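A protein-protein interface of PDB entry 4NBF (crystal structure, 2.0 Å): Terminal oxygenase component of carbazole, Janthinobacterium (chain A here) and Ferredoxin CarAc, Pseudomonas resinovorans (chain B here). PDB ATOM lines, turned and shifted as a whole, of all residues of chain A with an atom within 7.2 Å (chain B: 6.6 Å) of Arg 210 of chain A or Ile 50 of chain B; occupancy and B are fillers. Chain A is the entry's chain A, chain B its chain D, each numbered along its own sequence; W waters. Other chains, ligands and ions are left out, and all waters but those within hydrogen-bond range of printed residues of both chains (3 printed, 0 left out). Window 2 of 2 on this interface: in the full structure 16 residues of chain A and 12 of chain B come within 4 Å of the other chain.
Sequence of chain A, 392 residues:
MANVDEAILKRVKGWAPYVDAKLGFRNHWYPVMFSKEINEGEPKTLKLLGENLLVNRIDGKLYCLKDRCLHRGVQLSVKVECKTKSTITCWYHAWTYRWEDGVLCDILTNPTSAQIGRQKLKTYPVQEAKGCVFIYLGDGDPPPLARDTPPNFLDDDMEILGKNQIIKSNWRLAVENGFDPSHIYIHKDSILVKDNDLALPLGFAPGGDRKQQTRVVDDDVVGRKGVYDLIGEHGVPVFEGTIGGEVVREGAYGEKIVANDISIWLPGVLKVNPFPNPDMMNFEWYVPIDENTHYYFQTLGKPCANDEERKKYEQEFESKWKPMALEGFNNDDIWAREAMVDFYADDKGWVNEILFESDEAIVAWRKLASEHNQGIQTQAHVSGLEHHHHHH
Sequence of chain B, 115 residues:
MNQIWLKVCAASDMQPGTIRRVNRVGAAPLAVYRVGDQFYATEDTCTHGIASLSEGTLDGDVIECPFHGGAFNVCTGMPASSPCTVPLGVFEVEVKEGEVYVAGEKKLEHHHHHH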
ATOM      1  N   TRP A  15      15.551  30.704  11.107  1.00  0.00           N
ATOM      2  CA  TRP A  15      16.432  31.291  12.110  1.00  0.00           C
ATOM      3  C   TRP A  15      16.899  32.716  11.814  1.00  0.00           C
ATOM      4  O   TRP A  15      18.091  33.032  11.942  1.00  0.00           O
ATOM      5  CB  TRP A  15      17.635  30.361  12.301  1.00  0.00           C
ATOM      6  CG  TRP A  15      18.288  29.914  11.005  1.00  0.00           C
ATOM      7  CD1 TRP A  15      19.165  30.627  10.241  1.00  0.00           C
ATOM      8  CD2 TRP A  15      18.118  28.649  10.344  1.00  0.00           C
ATOM      9  NE1 TRP A  15      19.558  29.885   9.147  1.00  0.00           N
ATOM     10  CE2 TRP A  15      18.928  28.669   9.187  1.00  0.00           C
ATOM     11  CE3 TRP A  15      17.361  27.501  10.620  1.00  0.00           C
ATOM     12  CZ2 TRP A  15      19.005  27.582   8.303  1.00  0.00           C
ATOM     13  CZ3 TRP A  15      17.437  26.422   9.739  1.00  0.00           C
ATOM     14  CH2 TRP A  15      18.254  26.471   8.596  1.00  0.00           C
ATOM     15  N   GLY A 207      21.916   7.470  11.711  1.00  0.00           N
ATOM     16  CA  GLY A 207      20.982   6.377  11.914  1.00  0.00           C
ATOM     17  C   GLY A 207      19.779   6.910  12.678  1.00  0.00           C
ATOM     18  O   GLY A 207      19.914   7.846  13.466  1.00  0.00           O
ATOM     19  N   GLY A 208      18.602   6.329  12.450  1.00  0.00           N
ATOM     20  CA  GLY A 208      17.402   6.787  13.139  1.00  0.00           C
ATOM     21  C   GLY A 208      16.804   8.025  12.486  1.00  0.00           C
ATOM     22  O   GLY A 208      17.301   8.480  11.456  1.00  0.00           O
ATOM     23  N   ASP A 209      15.742   8.575  13.069  1.00  0.00           N
ATOM     24  CA  ASP A 209      15.117   9.767  12.500  1.00  0.00           C
ATOM     25  C   ASP A 209      15.919  11.011  12.872  1.00  0.00           C
ATOM     26  O   ASP A 209      16.701  10.990  13.823  1.00  0.00           O
ATOM     27  CB  ASP A 209      13.660   9.909  12.975  1.00  0.00           C
ATOM     28  CG  ASP A 209      13.524   9.907  14.489  1.00  0.00           C
ATOM     29  OD1 ASP A 209      14.285  10.629  15.162  1.00  0.00           O
ATOM     30  OD2 ASP A 209      12.641   9.190  15.010  1.00  0.00           O
ATOM     31  N   ARG A 210      15.728  12.090  12.121  1.00  0.00           N
ATOM     32  CA  ARG A 210      16.460  13.325  12.379  1.00  0.00           C
ATOM     33  C   ARG A 210      16.140  13.861  13.767  1.00  0.00           C
ATOM     34  O   ARG A 210      16.943  14.569  14.376  1.00  0.00           O
ATOM     35  CB  ARG A 210      16.124  14.385  11.323  1.00  0.00           C
ATOM     36  CG  ARG A 210      14.912  15.253  11.648  1.00  0.00           C
ATOM     37  CD  ARG A 210      14.753  16.379  10.629  1.00  0.00           C
ATOM     38  NE  ARG A 210      13.743  17.358  11.036  1.00  0.00           N
ATOM     39  CZ  ARG A 210      13.312  18.355  10.265  1.00  0.00           C
ATOM     40  NH1 ARG A 210      13.804  18.505   9.040  1.00  0.00           N
ATOM     41  NH2 ARG A 210      12.389  19.201  10.714  1.00  0.00           N
ATOM     42  N   LYS A 211      14.959  13.516  14.264  1.00  0.00           N
ATOM     43  CA  LYS A 211      14.532  13.963  15.578  1.00  0.00           C
ATOM     44  C   LYS A 211      15.444  13.354  16.639  1.00  0.00           C
ATOM     45  O   LYS A 211      15.630  13.919  17.715  1.00  0.00           O
ATOM     46  CB  LYS A 211      13.085  13.536  15.820  1.00  0.00           C
ATOM     47  CG  LYS A 211      12.197  13.671  14.585  1.00  0.00           C
ATOM     48  CD  LYS A 211      10.723  13.548  14.938  1.00  0.00           C
ATOM     49  CE  LYS A 211      10.289  14.688  15.848  1.00  0.00           C
ATOM     50  NZ  LYS A 211       8.836  14.628  16.170  1.00  0.00           N
ATOM     51  N   GLN A 212      16.017  12.198  16.317  1.00  0.00           N
ATOM     52  CA  GLN A 212      16.912  11.493  17.228  1.00  0.00           C
ATOM     53  C   GLN A 212      18.359  11.963  17.102  1.00  0.00           C
ATOM     54  O   GLN A 212      19.215  11.537  17.875  1.00  0.00           O
ATOM     55  CB  GLN A 212      16.871   9.987  16.954  1.00  0.00           C
ATOM     56  CG  GLN A 212      15.614   9.276  17.416  1.00  0.00           C
ATOM     57  CD  GLN A 212      15.581   7.828  16.958  1.00  0.00           C
ATOM     58  OE1 GLN A 212      15.537   7.541  15.755  1.00  0.00           O
ATOM     59  NE2 GLN A 212      15.610   6.904  17.916  1.00  0.00           N
ATOM     60  N   GLN A 213      18.629  12.832  16.135  1.00  0.00           N
ATOM     61  CA  GLN A 213      19.991  13.321  15.910  1.00  0.00           C
ATOM     62  C   GLN A 213      20.483  14.302  16.964  1.00  0.00           C
ATOM     63  O   GLN A 213      21.688  14.465  17.159  1.00  0.00           O
ATOM     64  CB  GLN A 213      20.098  13.980  14.533  1.00  0.00           C
ATOM     65  CG  GLN A 213      19.718  13.076  13.381  1.00  0.00           C
ATOM     66  CD  GLN A 213      20.433  11.744  13.433  1.00  0.00           C
ATOM     67  OE1 GLN A 213      21.668  11.684  13.442  1.00  0.00           O
ATOM     68  NE2 GLN A 213      19.662  10.662  13.471  1.00  0.00           N
ATOM     69  N   THR A 214      19.551  14.957  17.640  1.00  0.00           N
ATOM     70  CA  THR A 214      19.907  15.934  18.658  1.00  0.00           C
ATOM     71  C   THR A 214      18.935  15.886  19.820  1.00  0.00           C
ATOM     72  O   THR A 214      17.883  15.250  19.738  1.00  0.00           O
ATOM     73  CB  THR A 214      19.858  17.368  18.090  1.00  0.00           C
ATOM     74  OG1 THR A 214      18.515  17.671  17.691  1.00  0.00           O
ATOM     75  CG2 THR A 214      20.774  17.502  16.887  1.00  0.00           C
ATOM     76  N   ILE A 354      25.062  24.689   1.173  1.00  0.00           N
ATOM     77  CA  ILE A 354      24.367  23.448   0.833  1.00  0.00           C
ATOM     78  C   ILE A 354      24.677  22.479   1.971  1.00  0.00           C
ATOM     79  O   ILE A 354      25.757  21.887   2.031  1.00  0.00           O
ATOM     80  CB  ILE A 354      24.850  22.847  -0.508  1.00  0.00           C
ATOM     81  CG1 ILE A 354      24.482  23.791  -1.663  1.00  0.00           C
ATOM     82  CG2 ILE A 354      24.208  21.481  -0.717  1.00  0.00           C
ATOM     83  CD1 ILE A 354      24.987  23.340  -3.023  1.00  0.00           C
ATOM     84  N   LEU A 355      23.718  22.321   2.874  1.00  0.00           N
ATOM     85  CA  LEU A 355      23.885  21.470   4.045  1.00  0.00           C
ATOM     86  C   LEU A 355      23.636  19.989   3.788  1.00  0.00           C
ATOM     87  O   LEU A 355      22.942  19.625   2.840  1.00  0.00           O
ATOM     88  CB  LEU A 355      22.934  21.941   5.151  1.00  0.00           C
ATOM     89  CG  LEU A 355      22.909  23.448   5.425  1.00  0.00           C
ATOM     90  CD1 LEU A 355      21.935  23.748   6.553  1.00  0.00           C
ATOM     91  CD2 LEU A 355      24.306  23.930   5.776  1.00  0.00           C
ATOM     92  N   PHE A 356      24.226  19.135   4.621  1.00  0.00           N
ATOM     93  CA  PHE A 356      23.978  17.711   4.497  1.00  0.00           C
ATOM     94  C   PHE A 356      23.575  17.152   5.860  1.00  0.00           C
ATOM     95  O   PHE A 356      23.495  17.903   6.838  1.00  0.00           O
ATOM     96  CB  PHE A 356      25.149  16.964   3.796  1.00  0.00           C
ATOM     97  CG  PHE A 356      26.382  16.709   4.639  1.00  0.00           C
ATOM     98  CD1 PHE A 356      26.871  17.648   5.538  1.00  0.00           C
ATOM     99  CD2 PHE A 356      27.125  15.543   4.423  1.00  0.00           C
ATOM    100  CE1 PHE A 356      28.088  17.438   6.207  1.00  0.00           C
ATOM    101  CE2 PHE A 356      28.342  15.321   5.082  1.00  0.00           C
ATOM    102  CZ  PHE A 356      28.825  16.270   5.976  1.00  0.00           C
ATOM    103  N   GLU A 357      23.291  15.857   5.926  1.00  0.00           N
ATOM    104  CA  GLU A 357      22.788  15.240   7.154  1.00  0.00           C
ATOM    105  C   GLU A 357      23.330  15.650   8.523  1.00  0.00           C
ATOM    106  O   GLU A 357      22.550  16.057   9.386  1.00  0.00           O
ATOM    107  CB  GLU A 357      22.827  13.711   7.019  1.00  0.00           C
ATOM    108  CG  GLU A 357      21.884  13.163   5.940  1.00  0.00           C
ATOM    109  CD  GLU A 357      22.467  13.230   4.530  1.00  0.00           C
ATOM    110  OE1 GLU A 357      23.633  13.651   4.370  1.00  0.00           O
ATOM    111  OE2 GLU A 357      21.756  12.849   3.577  1.00  0.00           O
ATOM    112  N   SER A 358      24.636  15.557   8.744  1.00  0.00           N
ATOM    113  CA  SER A 358      25.177  15.918  10.053  1.00  0.00           C
ATOM    114  C   SER A 358      24.882  17.362  10.478  1.00  0.00           C
ATOM    115  O   SER A 358      24.975  17.692  11.659  1.00  0.00           O
ATOM    116  CB  SER A 358      26.688  15.663  10.108  1.00  0.00           C
ATOM    117  OG  SER A 358      27.384  16.392   9.113  1.00  0.00           O
ATOM    118  N   ASP A 359      24.526  18.220   9.523  1.00  0.00           N
ATOM    119  CA  ASP A 359      24.223  19.614   9.843  1.00  0.00           C
ATOM    120  C   ASP A 359      22.916  19.787  10.631  1.00  0.00           C
ATOM    121  O   ASP A 359      22.546  20.908  10.987  1.00  0.00           O
ATOM    122  CB  ASP A 359      24.184  20.469   8.567  1.00  0.00           C
ATOM    123  CG  ASP A 359      25.561  20.640   7.931  1.00  0.00           C
ATOM    124  OD1 ASP A 359      26.539  20.882   8.677  1.00  0.00           O
ATOM    125  OD2 ASP A 359      25.669  20.541   6.690  1.00  0.00           O
ATOM    126  N   GLU A 360      22.211  18.689  10.897  1.00  0.00           N
ATOM    127  CA  GLU A 360      20.980  18.776  11.683  1.00  0.00           C
ATOM    128  C   GLU A 360      21.349  19.372  13.039  1.00  0.00           C
ATOM    129  O   GLU A 360      20.547  20.054  13.667  1.00  0.00           O
ATOM    130  CB  GLU A 360      20.360  17.388  11.902  1.00  0.00           C
ATOM    131  CG  GLU A 360      19.695  16.783  10.675  1.00  0.00           C
ATOM    132  CD  GLU A 360      18.399  17.480  10.300  1.00  0.00           C
ATOM    133  OE1 GLU A 360      17.997  18.434  11.011  1.00  0.00           O
ATOM    134  OE2 GLU A 360      17.775  17.066   9.294  1.00  0.00           O
ATOM    135  N   ALA A 361      22.577  19.112  13.484  1.00  0.00           N
ATOM    136  CA  ALA A 361      23.043  19.633  14.769  1.00  0.00           C
ATOM    137  C   ALA A 361      23.124  21.161  14.728  1.00  0.00           C
ATOM    138  O   ALA A 361      22.665  21.849  15.648  1.00  0.00           O
ATOM    139  CB  ALA A 361      24.409  19.046  15.102  1.00  0.00           C
ATOM    140  N   VAL A 363      21.595  23.150  12.577  1.00  0.00           N
ATOM    141  CA  VAL A 363      20.243  23.663  12.390  1.00  0.00           C
ATOM    142  C   VAL A 363      19.513  23.743  13.735  1.00  0.00           C
ATOM    143  O   VAL A 363      18.819  24.724  14.016  1.00  0.00           O
ATOM    144  CB  VAL A 363      19.445  22.759  11.419  1.00  0.00           C
ATOM    145  CG1 VAL A 363      17.954  23.063  11.512  1.00  0.00           C
ATOM    146  CG2 VAL A 363      19.934  22.987   9.997  1.00  0.00           C
ATOM    147  N   LYS A 367      18.123  27.270  15.451  1.00  0.00           N
ATOM    148  CA  LYS A 367      16.746  27.477  15.881  1.00  0.00           C
ATOM    149  C   LYS A 367      16.674  27.737  17.379  1.00  0.00           C
ATOM    150  O   LYS A 367      15.915  28.597  17.823  1.00  0.00           O
ATOM    151  CB  LYS A 367      15.878  26.271  15.510  1.00  0.00           C
ATOM    152  CG  LYS A 367      15.828  26.043  14.013  1.00  0.00           C
ATOM    153  CD  LYS A 367      14.721  25.087  13.605  1.00  0.00           C
ATOM    154  CE  LYS A 367      14.668  24.955  12.087  1.00  0.00           C
ATOM    155  NZ  LYS A 367      13.450  24.207  11.636  1.00  0.00           N
ATOM    156  N   ARG B  21       2.819  16.205   4.963  1.00  0.00           N
ATOM    157  CA  ARG B  21       3.995  15.350   4.908  1.00  0.00           C
ATOM    158  C   ARG B  21       3.614  13.885   5.056  1.00  0.00           C
ATOM    159  O   ARG B  21       2.812  13.526   5.915  1.00  0.00           O
ATOM    160  CB  ARG B  21       4.989  15.728   6.005  1.00  0.00           C
ATOM    161  CG  ARG B  21       6.151  14.756   6.113  1.00  0.00           C
ATOM    162  CD  ARG B  21       7.203  15.220   7.102  1.00  0.00           C
ATOM    163  NE  ARG B  21       8.204  14.180   7.320  1.00  0.00           N
ATOM    164  CZ  ARG B  21       9.374  14.374   7.921  1.00  0.00           C
ATOM    165  NH1 ARG B  21       9.701  15.579   8.370  1.00  0.00           N
ATOM    166  NH2 ARG B  21      10.213  13.358   8.076  1.00  0.00           N
ATOM    167  N   ASP B  44       9.926  15.100   0.148  1.00  0.00           N
ATOM    168  CA  ASP B  44       9.780  16.153   1.150  1.00  0.00           C
ATOM    169  C   ASP B  44      11.049  16.980   1.344  1.00  0.00           C
ATOM    170  O   ASP B  44      10.985  18.184   1.593  1.00  0.00           O
ATOM    171  CB  ASP B  44       9.369  15.552   2.498  1.00  0.00           C
ATOM    172  CG  ASP B  44       9.119  16.612   3.558  1.00  0.00           C
ATOM    173  OD1 ASP B  44       8.212  17.448   3.357  1.00  0.00           O
ATOM    174  OD2 ASP B  44       9.826  16.612   4.591  1.00  0.00           O
ATOM    175  N   THR B  45      12.198  16.331   1.219  1.00  0.00           N
ATOM    176  CA  THR B  45      13.472  17.003   1.421  1.00  0.00           C
ATOM    177  C   THR B  45      13.895  17.929   0.287  1.00  0.00           C
ATOM    178  O   THR B  45      13.980  17.526  -0.873  1.00  0.00           O
ATOM    179  CB  THR B  45      14.578  15.971   1.672  1.00  0.00           C
ATOM    180  OG1 THR B  45      14.159  15.083   2.717  1.00  0.00           O
ATOM    181  CG2 THR B  45      15.872  16.661   2.089  1.00  0.00           C
ATOM    182  N   CYS B  46      14.158  19.183   0.633  1.00  0.00           N
ATOM    183  CA  CYS B  46      14.588  20.166  -0.354  1.00  0.00           C
ATOM    184  C   CYS B  46      15.890  19.673  -0.983  1.00  0.00           C
ATOM    185  O   CYS B  46      16.770  19.188  -0.278  1.00  0.00           O
ATOM    186  CB  CYS B  46      14.809  21.516   0.325  1.00  0.00           C
ATOM    187  SG  CYS B  46      15.334  22.797  -0.798  1.00  0.00           S
ATOM    188  N   THR B  47      16.011  19.786  -2.305  1.00  0.00           N
ATOM    189  CA  THR B  47      17.216  19.327  -3.001  1.00  0.00           C
ATOM    190  C   THR B  47      18.440  20.184  -2.680  1.00  0.00           C
ATOM    191  O   THR B  47      19.574  19.785  -2.949  1.00  0.00           O
ATOM    192  CB  THR B  47      17.027  19.324  -4.544  1.00  0.00           C
ATOM    193  OG1 THR B  47      16.910  20.670  -5.019  1.00  0.00           O
ATOM    194  CG2 THR B  47      15.761  18.552  -4.936  1.00  0.00           C
ATOM    195  N   HIS B  48      18.211  21.357  -2.099  1.00  0.00           N
ATOM    196  CA  HIS B  48      19.305  22.268  -1.756  1.00  0.00           C
ATOM    197  C   HIS B  48      19.912  22.013  -0.375  1.00  0.00           C
ATOM    198  O   HIS B  48      20.955  22.575  -0.039  1.00  0.00           O
ATOM    199  CB  HIS B  48      18.807  23.717  -1.857  1.00  0.00           C
ATOM    200  CG  HIS B  48      19.823  24.745  -1.466  1.00  0.00           C
ATOM    201  ND1 HIS B  48      19.715  25.496  -0.316  1.00  0.00           N
ATOM    202  CD2 HIS B  48      20.956  25.163  -2.083  1.00  0.00           C
ATOM    203  CE1 HIS B  48      20.734  26.336  -0.242  1.00  0.00           C
ATOM    204  NE2 HIS B  48      21.502  26.154  -1.302  1.00  0.00           N
ATOM    205  N   GLY B  49      19.272  21.168   0.428  1.00  0.00           N
ATOM    206  CA  GLY B  49      19.806  20.889   1.751  1.00  0.00           C
ATOM    207  C   GLY B  49      19.167  19.718   2.471  1.00  0.00           C
ATOM    208  O   GLY B  49      19.140  18.597   1.960  1.00  0.00           O
ATOM    209  N   ILE B  50      18.665  19.976   3.673  1.00  0.00           N
ATOM    210  CA  ILE B  50      18.025  18.939   4.473  1.00  0.00           C
ATOM    211  C   ILE B  50      16.684  19.406   5.036  1.00  0.00           C
ATOM    212  O   ILE B  50      16.090  18.744   5.889  1.00  0.00           O
ATOM    213  CB  ILE B  50      18.928  18.504   5.650  1.00  0.00           C
ATOM    214  CG1 ILE B  50      19.304  19.720   6.506  1.00  0.00           C
ATOM    215  CG2 ILE B  50      20.162  17.791   5.115  1.00  0.00           C
ATOM    216  CD1 ILE B  50      20.114  19.376   7.753  1.00  0.00           C
ATOM    217  N   ALA B  51      16.207  20.545   4.550  1.00  0.00           N
ATOM    218  CA  ALA B  51      14.936  21.089   5.011  1.00  0.00           C
ATOM    219  C   ALA B  51      13.741  20.253   4.560  1.00  0.00           C
ATOM    220  O   ALA B  51      13.803  19.545   3.553  1.00  0.00           O
ATOM    221  CB  ALA B  51      14.774  22.505   4.508  1.00  0.00           C
ATOM    222  N   SER B  52      12.658  20.343   5.323  1.00  0.00           N
ATOM    223  CA  SER B  52      11.423  19.642   5.001  1.00  0.00           C
ATOM    224  C   SER B  52      10.496  20.648   4.322  1.00  0.00           C
ATOM    225  O   SER B  52      10.050  21.612   4.945  1.00  0.00           O
ATOM    226  CB  SER B  52      10.759  19.109   6.270  1.00  0.00           C
ATOM    227  OG  SER B  52       9.414  18.751   6.008  1.00  0.00           O
ATOM    228  N   GLU B  55       7.192  21.930   5.647  1.00  0.00           N
ATOM    229  CA  GLU B  55       7.233  22.961   6.678  1.00  0.00           C
ATOM    230  C   GLU B  55       7.377  24.315   5.998  1.00  0.00           C
ATOM    231  O   GLU B  55       7.560  25.338   6.655  1.00  0.00           O
ATOM    232  CB  GLU B  55       8.409  22.732   7.634  1.00  0.00           C
ATOM    233  CG  GLU B  55       8.166  21.622   8.646  1.00  0.00           C
ATOM    234  CD  GLU B  55       9.321  21.433   9.613  1.00  0.00           C
ATOM    235  OE1 GLU B  55       9.962  22.438   9.989  1.00  0.00           O
ATOM    236  OE2 GLU B  55       9.577  20.279  10.017  1.00  0.00           O
ATOM    237  N   PHE B  67      14.106  26.952   4.835  1.00  0.00           N
ATOM    238  CA  PHE B  67      15.506  27.214   5.150  1.00  0.00           C
ATOM    239  C   PHE B  67      16.105  28.456   4.503  1.00  0.00           C
ATOM    240  O   PHE B  67      16.548  29.373   5.200  1.00  0.00           O
ATOM    241  CB  PHE B  67      16.376  26.003   4.775  1.00  0.00           C
ATOM    242  CG  PHE B  67      16.514  24.974   5.871  1.00  0.00           C
ATOM    243  CD1 PHE B  67      15.536  24.833   6.852  1.00  0.00           C
ATOM    244  CD2 PHE B  67      17.601  24.105   5.885  1.00  0.00           C
ATOM    245  CE1 PHE B  67      15.638  23.837   7.833  1.00  0.00           C
ATOM    246  CE2 PHE B  67      17.712  23.106   6.860  1.00  0.00           C
ATOM    247  CZ  PHE B  67      16.727  22.973   7.832  1.00  0.00           C
HETATM  248  O   HOH W   1      16.245  19.816   9.166  1.00  0.00           O
HETATM  249  O   HOH W   2      21.436  24.080   2.285  1.00  0.00           O
HETATM  250  O   HOH W   3      14.298  16.728   7.237  1.00  0.00           O
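NH2 of Arg 210 of chain A lies within salt-bridge range of OE2 of Glu 55 of chain B (3.1 Å).
The side-chain carboxylate of Asp 359 of chain A sits at hydrogen-bond distance from the backbone NH of Phe 356 of chain A (2.9 Å). SG of Cys 46 of chain B lies close to N of His 48 of chain B (3.5 Å).
Phe 67 of chain B touches Trp 15 of chain A. NH1 of Arg 210 of chain A touches O of Ile 50 of chain B, at 3.9 Å. His 48 of chain B touches Ile 354 of chain A (O to CG2, 3.5 Å). Leu 355 of chain A touches Gly 49 of chain B (O to CA, 3.6 Å). CG2 of Ile 50 of chain B touches C of Phe 356 of chain A (3.6 Å). Ile 50 of chain B touches Glu 357 of chain A (CG2 to N, 3.8 Å). CD1 of Ile 50 of chain B touches CD of Glu 360 of chain A (3.6 Å). CG2 of Val 363 of chain A touches CE2 of Phe 67 of chain B, at 3.8 Å.
Of the printed residues of chain B, Trp 15 of chain A touches Phe 67. Arg 210 of chain A touches just these residues of chain B: Ile 50 (3.9 Å) and Glu 55 (3.1 Å). Of the printed residues of chain B, Val 363 of chain A touches Phe 67 (3.8 Å). Ile 50 of chain B touches just these residues of chain A: Arg 210, Phe 356, Glu 357 and Glu 360. Of the printed residues of chain A, Glu 55 of chain B touches Arg 210 (3.1 Å). The nearest residue of chain B that does not touch Arg 210 of chain A is Ser 52 of chain B (4.2 Å). The nearest printed residue of chain B that does not touch Glu 357 of chain A is Gly 49 of chain B (6.4 Å).
Of the 19 printed residues of chain A, 8 touch a printed residue of chain B. Hydrophobic or aromatic side chains of chain A that line the printed part of chain B: Trp 15, Ile 354 and Val 363. Hydrophobic or aromatic side chains of chain B within 4 Å of the printed part of chain A: His 48, Ile 50 and Phe 67. Among the printed residues, 9 pairs touch across the chains.
Water W3 lies within hydrogen-bond range of NH1 of Arg 210 of chain A and O of Ile 50 of chain B. Water W1 lies within hydrogen-bond range of the guanidinium group of Arg 210 of chain A (2.8 Å), the side-chain carboxylate of Glu 360 of chain A (2.9 Å) and the backbone carbonyl oxygen of Ile 50 of chain B (3.5 Å). Water W2 lies within hydrogen-bond range of O of His 48 of chain B (2.8 Å) and N of Leu 355 of chain A (2.9 Å).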
